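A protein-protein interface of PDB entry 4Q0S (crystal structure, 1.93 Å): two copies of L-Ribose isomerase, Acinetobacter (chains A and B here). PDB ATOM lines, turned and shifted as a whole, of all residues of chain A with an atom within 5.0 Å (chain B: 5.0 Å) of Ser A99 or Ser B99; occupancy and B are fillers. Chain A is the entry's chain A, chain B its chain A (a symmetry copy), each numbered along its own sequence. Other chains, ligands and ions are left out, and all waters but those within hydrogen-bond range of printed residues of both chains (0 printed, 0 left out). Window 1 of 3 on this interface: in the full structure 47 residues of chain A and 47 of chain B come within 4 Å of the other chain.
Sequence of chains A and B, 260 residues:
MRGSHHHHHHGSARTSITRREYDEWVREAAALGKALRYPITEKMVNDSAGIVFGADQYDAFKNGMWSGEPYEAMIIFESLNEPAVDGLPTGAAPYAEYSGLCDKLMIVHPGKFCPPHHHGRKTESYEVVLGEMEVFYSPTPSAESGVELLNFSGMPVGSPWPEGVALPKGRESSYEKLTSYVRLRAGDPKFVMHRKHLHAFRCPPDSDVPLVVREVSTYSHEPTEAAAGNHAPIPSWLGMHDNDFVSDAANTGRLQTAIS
OG of Ser A99 is in hydrogen-bond range of OG of Ser B99 (2.7 Å).
O of Ser A99 sits at hydrogen-bond distance from N of Tyr A219, 2.7 Å away. The backbone carbonyl oxygen (O) of Ser B99 is in hydrogen-bond range of the backbone NH (N) of Tyr B219, at 2.7 Å.
Among the printed residues, pairs that only touch across the chains: Tyr A95 with Tyr B95, Tyr A98 with Ser B99, Ser A99 with Tyr B98, Leu A101 with Leu B101, Leu A101 with Thr B218 and Thr A218 with Leu B101.
Of chain B, only Tyr B98 and Ser B99 come within 4 Å of Ser A99. Of the printed residues of chain A, Ser B99 touches Tyr A98 (3.8 Å) and Ser A99 (2.7 Å). Of the printed residues of chain B, Tyr A98 touches Ser B99. Of the printed residues of chain B, Thr A218 touches Leu B101 (3.9 Å). Printed residues of chain B within 4 Å of Tyr A95: Tyr B95. Printed residues of chain B within 4 Å of Leu A101: Leu B101 (3.8 Å) and Thr B218 (3.9 Å). Of the printed residues of chain A, Thr B218 touches Leu A101 (3.9 Å). The nearest printed residue of chain A that does not touch Tyr B95 is Ser A99 (6.4 Å).
Hydrophobic or aromatic side chains of chain B within 4 Å of the printed part of chain A: Tyr B95 and Leu B101.
Tyr A95 touches its own counterpart, Tyr B95. Tyr A98 touches Ser B99, and with the chains exchanged Ser A99 touches Tyr B98. Leu B101 touches its own counterpart, Leu A101. Leu A101 touches Thr B218, and with the chains exchanged Thr A218 touches Leu B101. Of the 7 pairs that touch across the chains among the printed residues, 7 have their exchanged pair printed and touching as well.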
ATOM      1  N   PRO A  83     -21.697 -23.338  -3.076  1.00  0.00           N
ATOM      2  CA  PRO A  83     -21.020 -23.351  -4.375  1.00  0.00           C
ATOM      3  C   PRO A  83     -20.144 -22.119  -4.584  1.00  0.00           C
ATOM      4  O   PRO A  83     -19.076 -22.210  -5.184  1.00  0.00           O
ATOM      5  CB  PRO A  83     -22.180 -23.405  -5.373  1.00  0.00           C
ATOM      6  CG  PRO A  83     -23.234 -24.167  -4.622  1.00  0.00           C
ATOM      7  CD  PRO A  83     -23.149 -23.526  -3.240  1.00  0.00           C
ATOM      8  N   ALA A  84     -20.598 -20.978  -4.069  1.00  0.00           N
ATOM      9  CA  ALA A  84     -19.878 -19.711  -4.218  1.00  0.00           C
ATOM     10  C   ALA A  84     -19.787 -19.347  -5.707  1.00  0.00           C
ATOM     11  O   ALA A  84     -18.791 -18.793  -6.177  1.00  0.00           O
ATOM     12  CB  ALA A  84     -18.486 -19.813  -3.609  1.00  0.00           C
ATOM     13  N   TYR A  95     -14.049 -23.648 -13.839  1.00  0.00           N
ATOM     14  CA  TYR A  95     -13.120 -23.828 -12.723  1.00  0.00           C
ATOM     15  C   TYR A  95     -13.756 -23.566 -11.358  1.00  0.00           C
ATOM     16  O   TYR A  95     -13.088 -23.650 -10.328  1.00  0.00           O
ATOM     17  CB  TYR A  95     -11.914 -22.906 -12.903  1.00  0.00           C
ATOM     18  CG  TYR A  95     -11.262 -23.024 -14.261  1.00  0.00           C
ATOM     19  CD1 TYR A  95     -10.611 -24.197 -14.644  1.00  0.00           C
ATOM     20  CD2 TYR A  95     -11.305 -21.965 -15.170  1.00  0.00           C
ATOM     21  CE1 TYR A  95     -10.016 -24.315 -15.897  1.00  0.00           C
ATOM     22  CE2 TYR A  95     -10.712 -22.070 -16.428  1.00  0.00           C
ATOM     23  CZ  TYR A  95     -10.069 -23.248 -16.784  1.00  0.00           C
ATOM     24  OH  TYR A  95      -9.475 -23.357 -18.021  1.00  0.00           O
ATOM     25  N   ALA A  96     -15.047 -23.252 -11.352  1.00  0.00           N
ATOM     26  CA  ALA A  96     -15.766 -22.971 -10.114  1.00  0.00           C
ATOM     27  C   ALA A  96     -15.797 -24.183  -9.181  1.00  0.00           C
ATOM     28  O   ALA A  96     -15.777 -24.037  -7.958  1.00  0.00           O
ATOM     29  CB  ALA A  96     -17.188 -22.525 -10.436  1.00  0.00           C
ATOM     30  N   GLU A  97     -15.842 -25.371  -9.774  1.00  0.00           N
ATOM     31  CA  GLU A  97     -15.890 -26.632  -9.043  1.00  0.00           C
ATOM     32  C   GLU A  97     -14.705 -26.841  -8.094  1.00  0.00           C
ATOM     33  O   GLU A  97     -14.742 -27.721  -7.237  1.00  0.00           O
ATOM     34  CB  GLU A  97     -15.964 -27.793 -10.038  1.00  0.00           C
ATOM     35  CG  GLU A  97     -14.772 -27.859 -10.990  1.00  0.00           C
ATOM     36  CD  GLU A  97     -15.041 -28.727 -12.204  1.00  0.00           C
ATOM     37  OE1 GLU A  97     -15.880 -28.330 -13.039  1.00  0.00           O
ATOM     38  OE2 GLU A  97     -14.420 -29.805 -12.318  1.00  0.00           O
ATOM     39  N   TYR A  98     -13.655 -26.042  -8.259  1.00  0.00           N
ATOM     40  CA  TYR A  98     -12.477 -26.154  -7.402  1.00  0.00           C
ATOM     41  C   TYR A  98     -12.605 -25.218  -6.207  1.00  0.00           C
ATOM     42  O   TYR A  98     -11.806 -25.286  -5.270  1.00  0.00           O
ATOM     43  CB  TYR A  98     -11.209 -25.805  -8.183  1.00  0.00           C
ATOM     44  CG  TYR A  98     -10.831 -26.822  -9.234  1.00  0.00           C
ATOM     45  CD1 TYR A  98     -10.147 -27.986  -8.889  1.00  0.00           C
ATOM     46  CD2 TYR A  98     -11.177 -26.631 -10.571  1.00  0.00           C
ATOM     47  CE1 TYR A  98      -9.812 -28.936  -9.852  1.00  0.00           C
ATOM     48  CE2 TYR A  98     -10.852 -27.574 -11.539  1.00  0.00           C
ATOM     49  CZ  TYR A  98     -10.170 -28.722 -11.174  1.00  0.00           C
ATOM     50  OH  TYR A  98      -9.858 -29.658 -12.128  1.00  0.00           O
ATOM     51  N   SER A  99     -13.607 -24.344  -6.252  1.00  0.00           N
ATOM     52  CA  SER A  99     -13.831 -23.389  -5.178  1.00  0.00           C
ATOM     53  C   SER A  99     -15.031 -23.791  -4.323  1.00  0.00           C
ATOM     54  O   SER A  99     -15.325 -24.977  -4.171  1.00  0.00           O
ATOM     55  CB  SER A  99     -14.034 -21.985  -5.753  1.00  0.00           C
ATOM     56  OG  SER A  99     -14.005 -21.006  -4.722  1.00  0.00           O
ATOM     57  N   GLY A 100     -15.728 -22.804  -3.770  1.00  0.00           N
ATOM     58  CA  GLY A 100     -16.867 -23.096  -2.922  1.00  0.00           C
ATOM     59  C   GLY A 100     -16.416 -23.203  -1.473  1.00  0.00           C
ATOM     60  O   GLY A 100     -15.215 -23.246  -1.193  1.00  0.00           O
ATOM     61  N   LEU A 101     -17.371 -23.256  -0.549  1.00  0.00           N
ATOM     62  CA  LEU A 101     -17.054 -23.347   0.874  1.00  0.00           C
ATOM     63  C   LEU A 101     -17.851 -24.457   1.559  1.00  0.00           C
ATOM     64  O   LEU A 101     -19.083 -24.466   1.531  1.00  0.00           O
ATOM     65  CB  LEU A 101     -17.337 -21.999   1.551  1.00  0.00           C
ATOM     66  CG  LEU A 101     -16.551 -20.800   1.002  1.00  0.00           C
ATOM     67  CD1 LEU A 101     -17.180 -19.508   1.486  1.00  0.00           C
ATOM     68  CD2 LEU A 101     -15.096 -20.889   1.429  1.00  0.00           C
ATOM     69  N   THR A 218     -13.135 -26.582   0.241  1.00  0.00           N
ATOM     70  CA  THR A 218     -13.804 -26.038  -0.925  1.00  0.00           C
ATOM     71  C   THR A 218     -15.028 -26.933  -1.113  1.00  0.00           C
ATOM     72  O   THR A 218     -15.166 -27.946  -0.418  1.00  0.00           O
ATOM     73  CB  THR A 218     -12.885 -26.067  -2.185  1.00  0.00           C
ATOM     74  OG1 THR A 218     -12.397 -27.392  -2.404  1.00  0.00           O
ATOM     75  CG2 THR A 218     -11.693 -25.132  -1.999  1.00  0.00           C
ATOM     76  N   TYR A 219     -15.905 -26.568  -2.041  1.00  0.00           N
ATOM     77  CA  TYR A 219     -17.141 -27.313  -2.278  1.00  0.00           C
ATOM     78  C   TYR A 219     -17.013 -28.834  -2.311  1.00  0.00           C
ATOM     79  O   TYR A 219     -16.080 -29.381  -2.896  1.00  0.00           O
ATOM     80  CB  TYR A 219     -17.790 -26.843  -3.579  1.00  0.00           C
ATOM     81  CG  TYR A 219     -19.213 -27.315  -3.756  1.00  0.00           C
ATOM     82  CD1 TYR A 219     -20.265 -26.684  -3.094  1.00  0.00           C
ATOM     83  CD2 TYR A 219     -19.513 -28.388  -4.597  1.00  0.00           C
ATOM     84  CE1 TYR A 219     -21.582 -27.107  -3.266  1.00  0.00           C
ATOM     85  CE2 TYR A 219     -20.830 -28.822  -4.781  1.00  0.00           C
ATOM     86  CZ  TYR A 219     -21.857 -28.175  -4.113  1.00  0.00           C
ATOM     87  OH  TYR A 219     -23.156 -28.583  -4.303  1.00  0.00           O
ATOM     88  N   PRO B  83      -4.545 -19.985  -0.149  1.00  0.00           N
ATOM     89  CA  PRO B  83      -4.820 -19.671  -1.553  1.00  0.00           C
ATOM     90  C   PRO B  83      -5.558 -20.800  -2.265  1.00  0.00           C
ATOM     91  O   PRO B  83      -6.410 -20.548  -3.112  1.00  0.00           O
ATOM     92  CB  PRO B  83      -3.424 -19.441  -2.139  1.00  0.00           C
ATOM     93  CG  PRO B  83      -2.655 -18.892  -0.971  1.00  0.00           C
ATOM     94  CD  PRO B  83      -3.114 -19.812   0.157  1.00  0.00           C
ATOM     95  N   ALA B  84      -5.235 -22.039  -1.899  1.00  0.00           N
ATOM     96  CA  ALA B  84      -5.840 -23.221  -2.518  1.00  0.00           C
ATOM     97  C   ALA B  84      -5.487 -23.253  -4.012  1.00  0.00           C
ATOM     98  O   ALA B  84      -6.288 -23.661  -4.856  1.00  0.00           O
ATOM     99  CB  ALA B  84      -7.352 -23.207  -2.329  1.00  0.00           C
ATOM    100  N   TYR B  95      -8.776 -17.123 -12.328  1.00  0.00           N
ATOM    101  CA  TYR B  95      -9.993 -17.157 -11.516  1.00  0.00           C
ATOM    102  C   TYR B  95      -9.768 -17.727 -10.114  1.00  0.00           C
ATOM    103  O   TYR B  95     -10.707 -17.845  -9.328  1.00  0.00           O
ATOM    104  CB  TYR B  95     -11.066 -17.980 -12.229  1.00  0.00           C
ATOM    105  CG  TYR B  95     -11.303 -17.551 -13.659  1.00  0.00           C
ATOM    106  CD1 TYR B  95     -11.853 -16.303 -13.951  1.00  0.00           C
ATOM    107  CD2 TYR B  95     -10.966 -18.391 -14.722  1.00  0.00           C
ATOM    108  CE1 TYR B  95     -12.066 -15.900 -15.266  1.00  0.00           C
ATOM    109  CE2 TYR B  95     -11.174 -17.999 -16.044  1.00  0.00           C
ATOM    110  CZ  TYR B  95     -11.725 -16.752 -16.308  1.00  0.00           C
ATOM    111  OH  TYR B  95     -11.941 -16.361 -17.610  1.00  0.00           O
ATOM    112  N   ALA B  96      -8.524 -18.076  -9.805  1.00  0.00           N
ATOM    113  CA  ALA B  96      -8.183 -18.639  -8.503  1.00  0.00           C
ATOM    114  C   ALA B  96      -8.461 -17.658  -7.362  1.00  0.00           C
ATOM    115  O   ALA B  96      -8.828 -18.063  -6.259  1.00  0.00           O
ATOM    116  CB  ALA B  96      -6.716 -19.050  -8.490  1.00  0.00           C
ATOM    117  N   GLU B  97      -8.285 -16.372  -7.648  1.00  0.00           N
ATOM    118  CA  GLU B  97      -8.490 -15.300  -6.680  1.00  0.00           C
ATOM    119  C   GLU B  97      -9.905 -15.262  -6.091  1.00  0.00           C
ATOM    120  O   GLU B  97     -10.144 -14.589  -5.092  1.00  0.00           O
ATOM    121  CB  GLU B  97      -8.171 -13.955  -7.338  1.00  0.00           C
ATOM    122  CG  GLU B  97      -9.040 -13.648  -8.555  1.00  0.00           C
ATOM    123  CD  GLU B  97      -8.461 -12.548  -9.424  1.00  0.00           C
ATOM    124  OE1 GLU B  97      -7.404 -12.783 -10.048  1.00  0.00           O
ATOM    125  OE2 GLU B  97      -9.057 -11.452  -9.478  1.00  0.00           O
ATOM    126  N   TYR B  98     -10.837 -15.973  -6.719  1.00  0.00           N
ATOM    127  CA  TYR B  98     -12.214 -16.010  -6.234  1.00  0.00           C
ATOM    128  C   TYR B  98     -12.406 -17.185  -5.284  1.00  0.00           C
ATOM    129  O   TYR B  98     -13.443 -17.295  -4.625  1.00  0.00           O
ATOM    130  CB  TYR B  98     -13.192 -16.142  -7.404  1.00  0.00           C
ATOM    131  CG  TYR B  98     -13.283 -14.911  -8.274  1.00  0.00           C
ATOM    132  CD1 TYR B  98     -14.075 -13.828  -7.899  1.00  0.00           C
ATOM    133  CD2 TYR B  98     -12.561 -14.822  -9.464  1.00  0.00           C
ATOM    134  CE1 TYR B  98     -14.149 -12.683  -8.690  1.00  0.00           C
ATOM    135  CE2 TYR B  98     -12.624 -13.683 -10.258  1.00  0.00           C
ATOM    136  CZ  TYR B  98     -13.419 -12.619  -9.866  1.00  0.00           C
ATOM    137  OH  TYR B  98     -13.472 -11.490 -10.646  1.00  0.00           O
ATOM    138  N   SER B  99     -11.406 -18.061  -5.225  1.00  0.00           N
ATOM    139  CA  SER B  99     -11.470 -19.230  -4.364  1.00  0.00           C
ATOM    140  C   SER B  99     -10.581 -19.061  -3.134  1.00  0.00           C
ATOM    141  O   SER B  99     -10.381 -17.945  -2.652  1.00  0.00           O
ATOM    142  CB  SER B  99     -11.065 -20.484  -5.144  1.00  0.00           C
ATOM    143  OG  SER B  99     -11.359 -21.660  -4.400  1.00  0.00           O
ATOM    144  N   GLY B 100     -10.041 -20.166  -2.630  1.00  0.00           N
ATOM    145  CA  GLY B 100      -9.204 -20.099  -1.447  1.00  0.00           C
ATOM    146  C   GLY B 100     -10.056 -20.291  -0.202  1.00  0.00           C
ATOM    147  O   GLY B 100     -11.288 -20.271  -0.278  1.00  0.00           O
ATOM    148  N   LEU B 101      -9.410 -20.470   0.946  1.00  0.00           N
ATOM    149  CA  LEU B 101     -10.127 -20.676   2.203  1.00  0.00           C
ATOM    150  C   LEU B 101      -9.596 -19.766   3.310  1.00  0.00           C
ATOM    151  O   LEU B 101      -8.409 -19.790   3.640  1.00  0.00           O
ATOM    152  CB  LEU B 101     -10.007 -22.146   2.626  1.00  0.00           C
ATOM    153  CG  LEU B 101     -10.563 -23.174   1.629  1.00  0.00           C
ATOM    154  CD1 LEU B 101     -10.059 -24.560   1.985  1.00  0.00           C
ATOM    155  CD2 LEU B 101     -12.081 -23.132   1.629  1.00  0.00           C
ATOM    156  N   THR B 218     -13.798 -17.257   1.179  1.00  0.00           N
ATOM    157  CA  THR B 218     -12.805 -17.559   0.166  1.00  0.00           C
ATOM    158  C   THR B 218     -11.609 -16.684   0.536  1.00  0.00           C
ATOM    159  O   THR B 218     -11.708 -15.849   1.442  1.00  0.00           O
ATOM    160  CB  THR B 218     -13.323 -17.230  -1.268  1.00  0.00           C
ATOM    161  OG1 THR B 218     -13.770 -15.874  -1.328  1.00  0.00           O
ATOM    162  CG2 THR B 218     -14.488 -18.144  -1.638  1.00  0.00           C
ATOM    163  N   TYR B 219     -10.490 -16.868  -0.156  1.00  0.00           N
ATOM    164  CA  TYR B 219      -9.263 -16.130   0.139  1.00  0.00           C
ATOM    165  C   TYR B 219      -9.425 -14.635   0.398  1.00  0.00           C
ATOM    166  O   TYR B 219     -10.166 -13.945  -0.299  1.00  0.00           O
ATOM    167  CB  TYR B 219      -8.252 -16.330  -0.989  1.00  0.00           C
ATOM    168  CG  TYR B 219      -6.854 -15.877  -0.643  1.00  0.00           C
ATOM    169  CD1 TYR B 219      -6.018 -16.669   0.142  1.00  0.00           C
ATOM    170  CD2 TYR B 219      -6.359 -14.658  -1.111  1.00  0.00           C
ATOM    171  CE1 TYR B 219      -4.721 -16.261   0.452  1.00  0.00           C
ATOM    172  CE2 TYR B 219      -5.060 -14.237  -0.810  1.00  0.00           C
ATOM    173  CZ  TYR B 219      -4.248 -15.045  -0.030  1.00  0.00           C
ATOM    174  OH  TYR B 219      -2.963 -14.648   0.254  1.00  0.00           O
